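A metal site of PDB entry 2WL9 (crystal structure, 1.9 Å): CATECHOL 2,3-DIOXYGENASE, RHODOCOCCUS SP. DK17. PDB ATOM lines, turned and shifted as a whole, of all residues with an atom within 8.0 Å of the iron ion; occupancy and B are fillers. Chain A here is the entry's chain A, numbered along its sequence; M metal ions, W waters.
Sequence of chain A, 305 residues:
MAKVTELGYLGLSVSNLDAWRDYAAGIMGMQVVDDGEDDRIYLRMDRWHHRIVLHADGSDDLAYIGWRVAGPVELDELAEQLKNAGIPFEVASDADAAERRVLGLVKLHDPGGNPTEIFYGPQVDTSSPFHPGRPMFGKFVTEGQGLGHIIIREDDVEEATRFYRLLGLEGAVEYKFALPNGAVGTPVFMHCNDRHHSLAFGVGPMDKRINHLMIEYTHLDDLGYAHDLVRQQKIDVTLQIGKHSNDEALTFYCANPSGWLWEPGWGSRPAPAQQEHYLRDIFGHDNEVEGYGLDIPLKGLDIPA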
ATOM      1  N   HIS A 149      -0.150  15.235  24.844  1.00  0.00           N
ATOM      2  CA  HIS A 149      -1.480  14.688  24.581  1.00  0.00           C
ATOM      3  C   HIS A 149      -2.003  14.997  23.183  1.00  0.00           C
ATOM      4  O   HIS A 149      -1.540  15.931  22.520  1.00  0.00           O
ATOM      5  CB  HIS A 149      -2.496  15.054  25.679  1.00  0.00           C
ATOM      6  CG  HIS A 149      -2.976  16.481  25.648  1.00  0.00           C
ATOM      7  ND1 HIS A 149      -2.768  17.351  26.699  1.00  0.00           N
ATOM      8  CD2 HIS A 149      -3.670  17.177  24.717  1.00  0.00           C
ATOM      9  CE1 HIS A 149      -3.321  18.525  26.415  1.00  0.00           C
ATOM     10  NE2 HIS A 149      -3.873  18.445  25.216  1.00  0.00           N
ATOM     11  N   ILE A 150      -2.945  14.166  22.735  1.00  0.00           N
ATOM     12  CA  ILE A 150      -3.530  14.286  21.395  1.00  0.00           C
ATOM     13  C   ILE A 150      -5.056  14.248  21.461  1.00  0.00           C
ATOM     14  O   ILE A 150      -5.618  13.544  22.291  1.00  0.00           O
ATOM     15  CB  ILE A 150      -3.016  13.147  20.454  1.00  0.00           C
ATOM     16  CG1 ILE A 150      -3.224  11.760  21.072  1.00  0.00           C
ATOM     17  CG2 ILE A 150      -1.538  13.367  20.099  1.00  0.00           C
ATOM     18  CD1 ILE A 150      -2.893  10.586  20.140  1.00  0.00           C
ATOM     19  N   ILE A 151      -5.708  15.010  20.588  1.00  0.00           N
ATOM     20  CA  ILE A 151      -7.126  14.784  20.300  1.00  0.00           C
ATOM     21  C   ILE A 151      -7.220  14.031  18.964  1.00  0.00           C
ATOM     22  O   ILE A 151      -6.570  14.421  17.984  1.00  0.00           O
ATOM     23  CB  ILE A 151      -7.934  16.104  20.256  1.00  0.00           C
ATOM     24  CG1 ILE A 151      -8.129  16.630  21.686  1.00  0.00           C
ATOM     25  CG2 ILE A 151      -9.282  15.896  19.577  1.00  0.00           C
ATOM     26  CD1 ILE A 151      -9.153  17.738  21.852  1.00  0.00           C
ATOM     27  N   PHE A 189     -11.899  13.000  28.012  1.00  0.00           N
ATOM     28  CA  PHE A 189     -10.471  13.164  28.280  1.00  0.00           C
ATOM     29  C   PHE A 189     -10.006  11.992  29.125  1.00  0.00           C
ATOM     30  O   PHE A 189     -10.708  11.587  30.058  1.00  0.00           O
ATOM     31  CB  PHE A 189     -10.204  14.484  29.031  1.00  0.00           C
ATOM     32  CG  PHE A 189     -10.499  15.712  28.215  1.00  0.00           C
ATOM     33  CD1 PHE A 189      -9.478  16.397  27.577  1.00  0.00           C
ATOM     34  CD2 PHE A 189     -11.813  16.164  28.052  1.00  0.00           C
ATOM     35  CE1 PHE A 189      -9.749  17.535  26.805  1.00  0.00           C
ATOM     36  CE2 PHE A 189     -12.088  17.289  27.291  1.00  0.00           C
ATOM     37  CZ  PHE A 189     -11.057  17.977  26.661  1.00  0.00           C
ATOM     38  N   HIS A 197      -4.259  14.817  30.863  1.00  0.00           N
ATOM     39  CA  HIS A 197      -4.738  13.776  29.963  1.00  0.00           C
ATOM     40  C   HIS A 197      -3.683  13.508  28.904  1.00  0.00           C
ATOM     41  O   HIS A 197      -2.846  14.377  28.629  1.00  0.00           O
ATOM     42  CB  HIS A 197      -6.112  14.126  29.357  1.00  0.00           C
ATOM     43  CG  HIS A 197      -6.131  15.375  28.542  1.00  0.00           C
ATOM     44  ND1 HIS A 197      -6.270  16.636  29.089  1.00  0.00           N
ATOM     45  CD2 HIS A 197      -6.066  15.565  27.195  1.00  0.00           C
ATOM     46  CE1 HIS A 197      -6.274  17.544  28.124  1.00  0.00           C
ATOM     47  NE2 HIS A 197      -6.152  16.916  26.967  1.00  0.00           N
ATOM     48  N   ALA A 200      -7.834  12.633  24.133  1.00  0.00           N
ATOM     49  CA  ALA A 200      -9.200  13.142  24.161  1.00  0.00           C
ATOM     50  C   ALA A 200      -9.874  12.929  22.817  1.00  0.00           C
ATOM     51  O   ALA A 200      -9.204  12.769  21.795  1.00  0.00           O
ATOM     52  CB  ALA A 200      -9.205  14.626  24.511  1.00  0.00           C
ATOM     53  N   ASN A 211      -6.425  16.164  15.674  1.00  0.00           N
ATOM     54  CA  ASN A 211      -6.771  17.579  15.644  1.00  0.00           C
ATOM     55  C   ASN A 211      -5.597  18.403  16.114  1.00  0.00           C
ATOM     56  O   ASN A 211      -5.258  19.433  15.509  1.00  0.00           O
ATOM     57  CB  ASN A 211      -8.002  17.882  16.518  1.00  0.00           C
ATOM     58  CG  ASN A 211      -8.250  19.373  16.674  1.00  0.00           C
ATOM     59  OD1 ASN A 211      -8.739  20.044  15.760  1.00  0.00           O
ATOM     60  ND2 ASN A 211      -7.901  19.909  17.842  1.00  0.00           N
ATOM     61  N   HIS A 212      -4.992  17.944  17.208  1.00  0.00           N
ATOM     62  CA  HIS A 212      -3.810  18.590  17.760  1.00  0.00           C
ATOM     63  C   HIS A 212      -2.978  17.681  18.662  1.00  0.00           C
ATOM     64  O   HIS A 212      -3.449  16.638  19.147  1.00  0.00           O
ATOM     65  CB  HIS A 212      -4.156  19.901  18.485  1.00  0.00           C
ATOM     66  CG  HIS A 212      -4.690  19.712  19.873  1.00  0.00           C
ATOM     67  ND1 HIS A 212      -6.037  19.593  20.147  1.00  0.00           N
ATOM     68  CD2 HIS A 212      -4.060  19.681  21.070  1.00  0.00           C
ATOM     69  CE1 HIS A 212      -6.211  19.473  21.452  1.00  0.00           C
ATOM     70  NE2 HIS A 212      -5.030  19.523  22.031  1.00  0.00           N
ATOM     71  N   LEU A 213      -1.755  18.111  18.889  1.00  0.00           N
ATOM     72  CA  LEU A 213      -0.836  17.560  19.841  1.00  0.00           C
ATOM     73  C   LEU A 213      -0.456  18.683  20.793  1.00  0.00           C
ATOM     74  O   LEU A 213      -0.158  19.724  20.356  1.00  0.00           O
ATOM     75  CB  LEU A 213       0.439  17.128  19.169  1.00  0.00           C
ATOM     76  CG  LEU A 213       1.662  16.928  20.030  1.00  0.00           C
ATOM     77  CD1 LEU A 213       1.432  15.896  21.041  1.00  0.00           C
ATOM     78  CD2 LEU A 213       2.823  16.625  19.217  1.00  0.00           C
ATOM     79  N   MET A 214      -0.448  18.456  22.073  1.00  0.00           N
ATOM     80  CA  MET A 214       0.012  19.437  23.006  1.00  0.00           C
ATOM     81  C   MET A 214       1.392  19.022  23.538  1.00  0.00           C
ATOM     82  O   MET A 214       1.591  17.920  23.914  1.00  0.00           O
ATOM     83  CB  MET A 214      -0.990  19.691  24.119  1.00  0.00           C
ATOM     84  CG  MET A 214      -0.653  19.254  25.486  1.00  0.00           C
ATOM     85  SD  MET A 214       0.684  19.971  26.394  1.00  0.00           S
ATOM     86  CE  MET A 214       0.002  21.362  27.146  1.00  0.00           C
ATOM     87  N   ILE A 215       2.311  19.938  23.493  1.00  0.00           N
ATOM     88  CA  ILE A 215       3.650  19.757  23.947  1.00  0.00           C
ATOM     89  C   ILE A 215       3.884  20.733  25.114  1.00  0.00           C
ATOM     90  O   ILE A 215       3.435  21.826  25.069  1.00  0.00           O
ATOM     91  CB  ILE A 215       4.711  19.933  22.864  1.00  0.00           C
ATOM     92  CG1 ILE A 215       4.677  21.306  22.231  1.00  0.00           C
ATOM     93  CG2 ILE A 215       4.595  18.851  21.837  1.00  0.00           C
ATOM     94  CD1 ILE A 215       5.628  21.480  21.142  1.00  0.00           C
ATOM     95  N   HIS A 244      -7.512  26.264  29.647  1.00  0.00           N
ATOM     96  CA  HIS A 244      -8.673  25.390  29.771  1.00  0.00           C
ATOM     97  C   HIS A 244      -8.961  25.170  31.269  1.00  0.00           C
ATOM     98  O   HIS A 244      -8.043  25.246  32.100  1.00  0.00           O
ATOM     99  CB  HIS A 244      -8.441  24.060  29.064  1.00  0.00           C
ATOM    100  CG  HIS A 244      -8.299  24.161  27.575  1.00  0.00           C
ATOM    101  ND1 HIS A 244      -9.288  24.695  26.775  1.00  0.00           N
ATOM    102  CD2 HIS A 244      -7.300  23.783  26.741  1.00  0.00           C
ATOM    103  CE1 HIS A 244      -8.899  24.667  25.513  1.00  0.00           C
ATOM    104  NE2 HIS A 244      -7.709  24.104  25.463  1.00  0.00           N
ATOM    105  N   ASN A 246      -9.895  22.358  32.616  1.00  0.00           N
ATOM    106  CA  ASN A 246      -9.491  21.009  33.054  1.00  0.00           C
ATOM    107  C   ASN A 246      -8.010  20.861  33.434  1.00  0.00           C
ATOM    108  O   ASN A 246      -7.701  20.489  34.570  1.00  0.00           O
ATOM    109  CB  ASN A 246      -9.989  19.917  32.085  1.00  0.00           C
ATOM    110  CG  ASN A 246      -9.495  20.099  30.644  1.00  0.00           C
ATOM    111  OD1 ASN A 246      -8.918  21.120  30.292  1.00  0.00           O
ATOM    112  ND2 ASN A 246      -9.721  19.085  29.814  1.00  0.00           N
ATOM    113  N   ASP A 247      -7.111  21.178  32.498  1.00  0.00           N
ATOM    114  CA  ASP A 247      -5.675  21.018  32.733  1.00  0.00           C
ATOM    115  C   ASP A 247      -5.038  22.271  33.342  1.00  0.00           C
ATOM    116  O   ASP A 247      -3.929  22.212  33.871  1.00  0.00           O
ATOM    117  CB  ASP A 247      -4.919  20.575  31.466  1.00  0.00           C
ATOM    118  CG  ASP A 247      -5.071  21.545  30.293  1.00  0.00           C
ATOM    119  OD1 ASP A 247      -5.520  22.700  30.478  1.00  0.00           O
ATOM    120  OD2 ASP A 247      -4.737  21.155  29.158  1.00  0.00           O
ATOM    121  N   ALA A 249      -3.616  24.599  32.166  1.00  0.00           N
ATOM    122  CA  ALA A 249      -2.340  24.904  31.523  1.00  0.00           C
ATOM    123  C   ALA A 249      -2.451  26.226  30.779  1.00  0.00           C
ATOM    124  O   ALA A 249      -3.538  26.591  30.321  1.00  0.00           O
ATOM    125  CB  ALA A 249      -1.986  23.798  30.561  1.00  0.00           C
ATOM    126  N   THR A 251      -1.720  27.760  27.419  1.00  0.00           N
ATOM    127  CA  THR A 251      -1.433  27.245  26.080  1.00  0.00           C
ATOM    128  C   THR A 251      -1.963  28.154  24.962  1.00  0.00           C
ATOM    129  O   THR A 251      -2.865  28.957  25.189  1.00  0.00           O
ATOM    130  CB  THR A 251      -2.022  25.805  25.847  1.00  0.00           C
ATOM    131  OG1 THR A 251      -3.422  25.880  25.538  1.00  0.00           O
ATOM    132  CG2 THR A 251      -1.810  24.888  27.043  1.00  0.00           C
ATOM    133  N   PHE A 252      -1.381  28.018  23.771  1.00  0.00           N
ATOM    134  CA  PHE A 252      -2.035  28.507  22.562  1.00  0.00           C
ATOM    135  C   PHE A 252      -2.016  27.404  21.526  1.00  0.00           C
ATOM    136  O   PHE A 252      -1.281  26.427  21.678  1.00  0.00           O
ATOM    137  CB  PHE A 252      -1.386  29.795  22.035  1.00  0.00           C
ATOM    138  CG  PHE A 252      -0.021  29.615  21.431  1.00  0.00           C
ATOM    139  CD1 PHE A 252       0.136  29.587  20.048  1.00  0.00           C
ATOM    140  CD2 PHE A 252       1.114  29.513  22.236  1.00  0.00           C
ATOM    141  CE1 PHE A 252       1.394  29.437  19.485  1.00  0.00           C
ATOM    142  CE2 PHE A 252       2.378  29.357  21.679  1.00  0.00           C
ATOM    143  CZ  PHE A 252       2.519  29.315  20.298  1.00  0.00           C
ATOM    144  N   TYR A 253      -2.835  27.553  20.484  1.00  0.00           N
ATOM    145  CA  TYR A 253      -2.963  26.546  19.438  1.00  0.00           C
ATOM    146  C   TYR A 253      -2.621  27.194  18.102  1.00  0.00           C
ATOM    147  O   TYR A 253      -3.257  28.172  17.711  1.00  0.00           O
ATOM    148  CB  TYR A 253      -4.399  26.025  19.342  1.00  0.00           C
ATOM    149  CG  TYR A 253      -4.945  25.167  20.471  1.00  0.00           C
ATOM    150  CD1 TYR A 253      -5.204  23.802  20.271  1.00  0.00           C
ATOM    151  CD2 TYR A 253      -5.268  25.710  21.716  1.00  0.00           C
ATOM    152  CE1 TYR A 253      -5.736  23.008  21.286  1.00  0.00           C
ATOM    153  CE2 TYR A 253      -5.801  24.926  22.742  1.00  0.00           C
ATOM    154  CZ  TYR A 253      -6.032  23.574  22.523  1.00  0.00           C
ATOM    155  OH  TYR A 253      -6.561  22.802  23.539  1.00  0.00           O
ATOM    156  N   TRP A 262      -0.544  22.243  16.572  1.00  0.00           N
ATOM    157  CA  TRP A 262       0.214  21.980  17.787  1.00  0.00           C
ATOM    158  C   TRP A 262      -0.175  23.007  18.836  1.00  0.00           C
ATOM    159  O   TRP A 262      -0.460  24.162  18.502  1.00  0.00           O
ATOM    160  CB  TRP A 262       1.718  22.011  17.517  1.00  0.00           C
ATOM    161  CG  TRP A 262       2.242  20.715  17.009  1.00  0.00           C
ATOM    162  CD1 TRP A 262       1.523  19.696  16.442  1.00  0.00           C
ATOM    163  CD2 TRP A 262       3.613  20.291  16.972  1.00  0.00           C
ATOM    164  NE1 TRP A 262       2.344  18.679  16.086  1.00  0.00           N
ATOM    165  CE2 TRP A 262       3.644  19.009  16.397  1.00  0.00           C
ATOM    166  CE3 TRP A 262       4.818  20.867  17.389  1.00  0.00           C
ATOM    167  CZ2 TRP A 262       4.817  18.287  16.221  1.00  0.00           C
ATOM    168  CZ3 TRP A 262       5.996  20.158  17.202  1.00  0.00           C
ATOM    169  CH2 TRP A 262       5.981  18.881  16.630  1.00  0.00           C
ATOM    170  N   GLU A 263      -0.191  22.561  20.082  1.00  0.00           N
ATOM    171  CA  GLU A 263      -0.576  23.383  21.227  1.00  0.00           C
ATOM    172  C   GLU A 263       0.585  23.447  22.228  1.00  0.00           C
ATOM    173  O   GLU A 263       0.670  22.619  23.129  1.00  0.00           O
ATOM    174  CB  GLU A 263      -1.843  22.813  21.879  1.00  0.00           C
ATOM    175  CG  GLU A 263      -2.370  23.594  23.088  1.00  0.00           C
ATOM    176  CD  GLU A 263      -3.228  22.746  24.034  1.00  0.00           C
ATOM    177  OE1 GLU A 263      -3.359  21.521  23.795  1.00  0.00           O
ATOM    178  OE2 GLU A 263      -3.784  23.303  25.005  1.00  0.00           O
ATOM    179  N   HIS A 285      -7.759  32.045  25.264  1.00  0.00           N
ATOM    180  CA  HIS A 285      -8.155  31.060  24.254  1.00  0.00           C
ATOM    181  C   HIS A 285      -9.211  31.646  23.309  1.00  0.00           C
ATOM    182  O   HIS A 285     -10.093  30.936  22.826  1.00  0.00           O
ATOM    183  CB  HIS A 285      -8.671  29.763  24.893  1.00  0.00           C
ATOM    184  CG  HIS A 285      -7.587  28.834  25.359  1.00  0.00           C
ATOM    185  ND1 HIS A 285      -6.293  28.892  24.879  1.00  0.00           N
ATOM    186  CD2 HIS A 285      -7.615  27.812  26.243  1.00  0.00           C
ATOM    187  CE1 HIS A 285      -5.573  27.946  25.466  1.00  0.00           C
ATOM    188  NE2 HIS A 285      -6.353  27.282  26.292  1.00  0.00           N
ATOM    189  N   LEU A 294     -11.576  23.871  15.668  1.00  0.00           N
ATOM    190  CA  LEU A 294     -11.782  24.380  17.019  1.00  0.00           C
ATOM    191  C   LEU A 294     -12.594  25.682  16.999  1.00  0.00           C
ATOM    192  O   LEU A 294     -12.392  26.560  17.844  1.00  0.00           O
ATOM    193  CB  LEU A 294     -10.433  24.587  17.735  1.00  0.00           C
ATOM    194  CG  LEU A 294      -9.591  23.337  17.995  1.00  0.00           C
ATOM    195  CD1 LEU A 294      -8.330  23.707  18.760  1.00  0.00           C
ATOM    196  CD2 LEU A 294     -10.380  22.283  18.759  1.00  0.00           C
HETATM  197 FE    FE M   1      -5.181  20.339  24.391  1.00  0.00          FE
HETATM  198  O   HOH W   1      -4.950  21.546  26.536  1.00  0.00           O
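The backbone carbonyl oxygen of Glu 263 is in hydrogen-bond range of the backbone NH of Ile 215 (3.2 Å).
NE2 of His 244 sits at hydrogen-bond distance from OH of Tyr 253, at 2.6 Å.
The side-chain carboxylate (OE2) of Glu 263 is in hydrogen-bond range of the side-chain hydroxyl (OH) of Tyr 253, at 3.2 Å.
The backbone NH (N) of Glu 263 sits at hydrogen-bond distance from the backbone carbonyl oxygen (O) of Leu 213.
A ring nitrogen (ND1) of His 212 is in hydrogen-bond range of the side-chain amide nitrogen (ND2) of Asn 211 (3.0 Å).
ND1 of His 149 sits close to NE2 of His 197, 3.4 Å away.
N of Ile 151 is in hydrogen-bond range of O of His 212 (3.1 Å).
OG1 of Thr 251 lies within hydrogen-bond range of OE2 of Glu 263, 2.7 Å away.
The side-chain carboxylate (OE1) of Glu 263 binds the iron ion (2.3 Å).
NE2 of His 149 is bound to the iron ion (2.4 Å).
The iron ion is bound by water W1 (2.5 Å).
NE2 of His 212 is bound to the iron ion (2.5 Å).
The iron ion has four donor atoms within binding distance.
Merely in contact with the iron ion: Tyr 253 (2.9 Å).
Within 4 Å of the iron ion: His 149, His 212, Tyr 253 and Glu 263.
Water W1 lies within hydrogen-bond range of OE2 of Glu 263 and OD2 of Asp 247.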
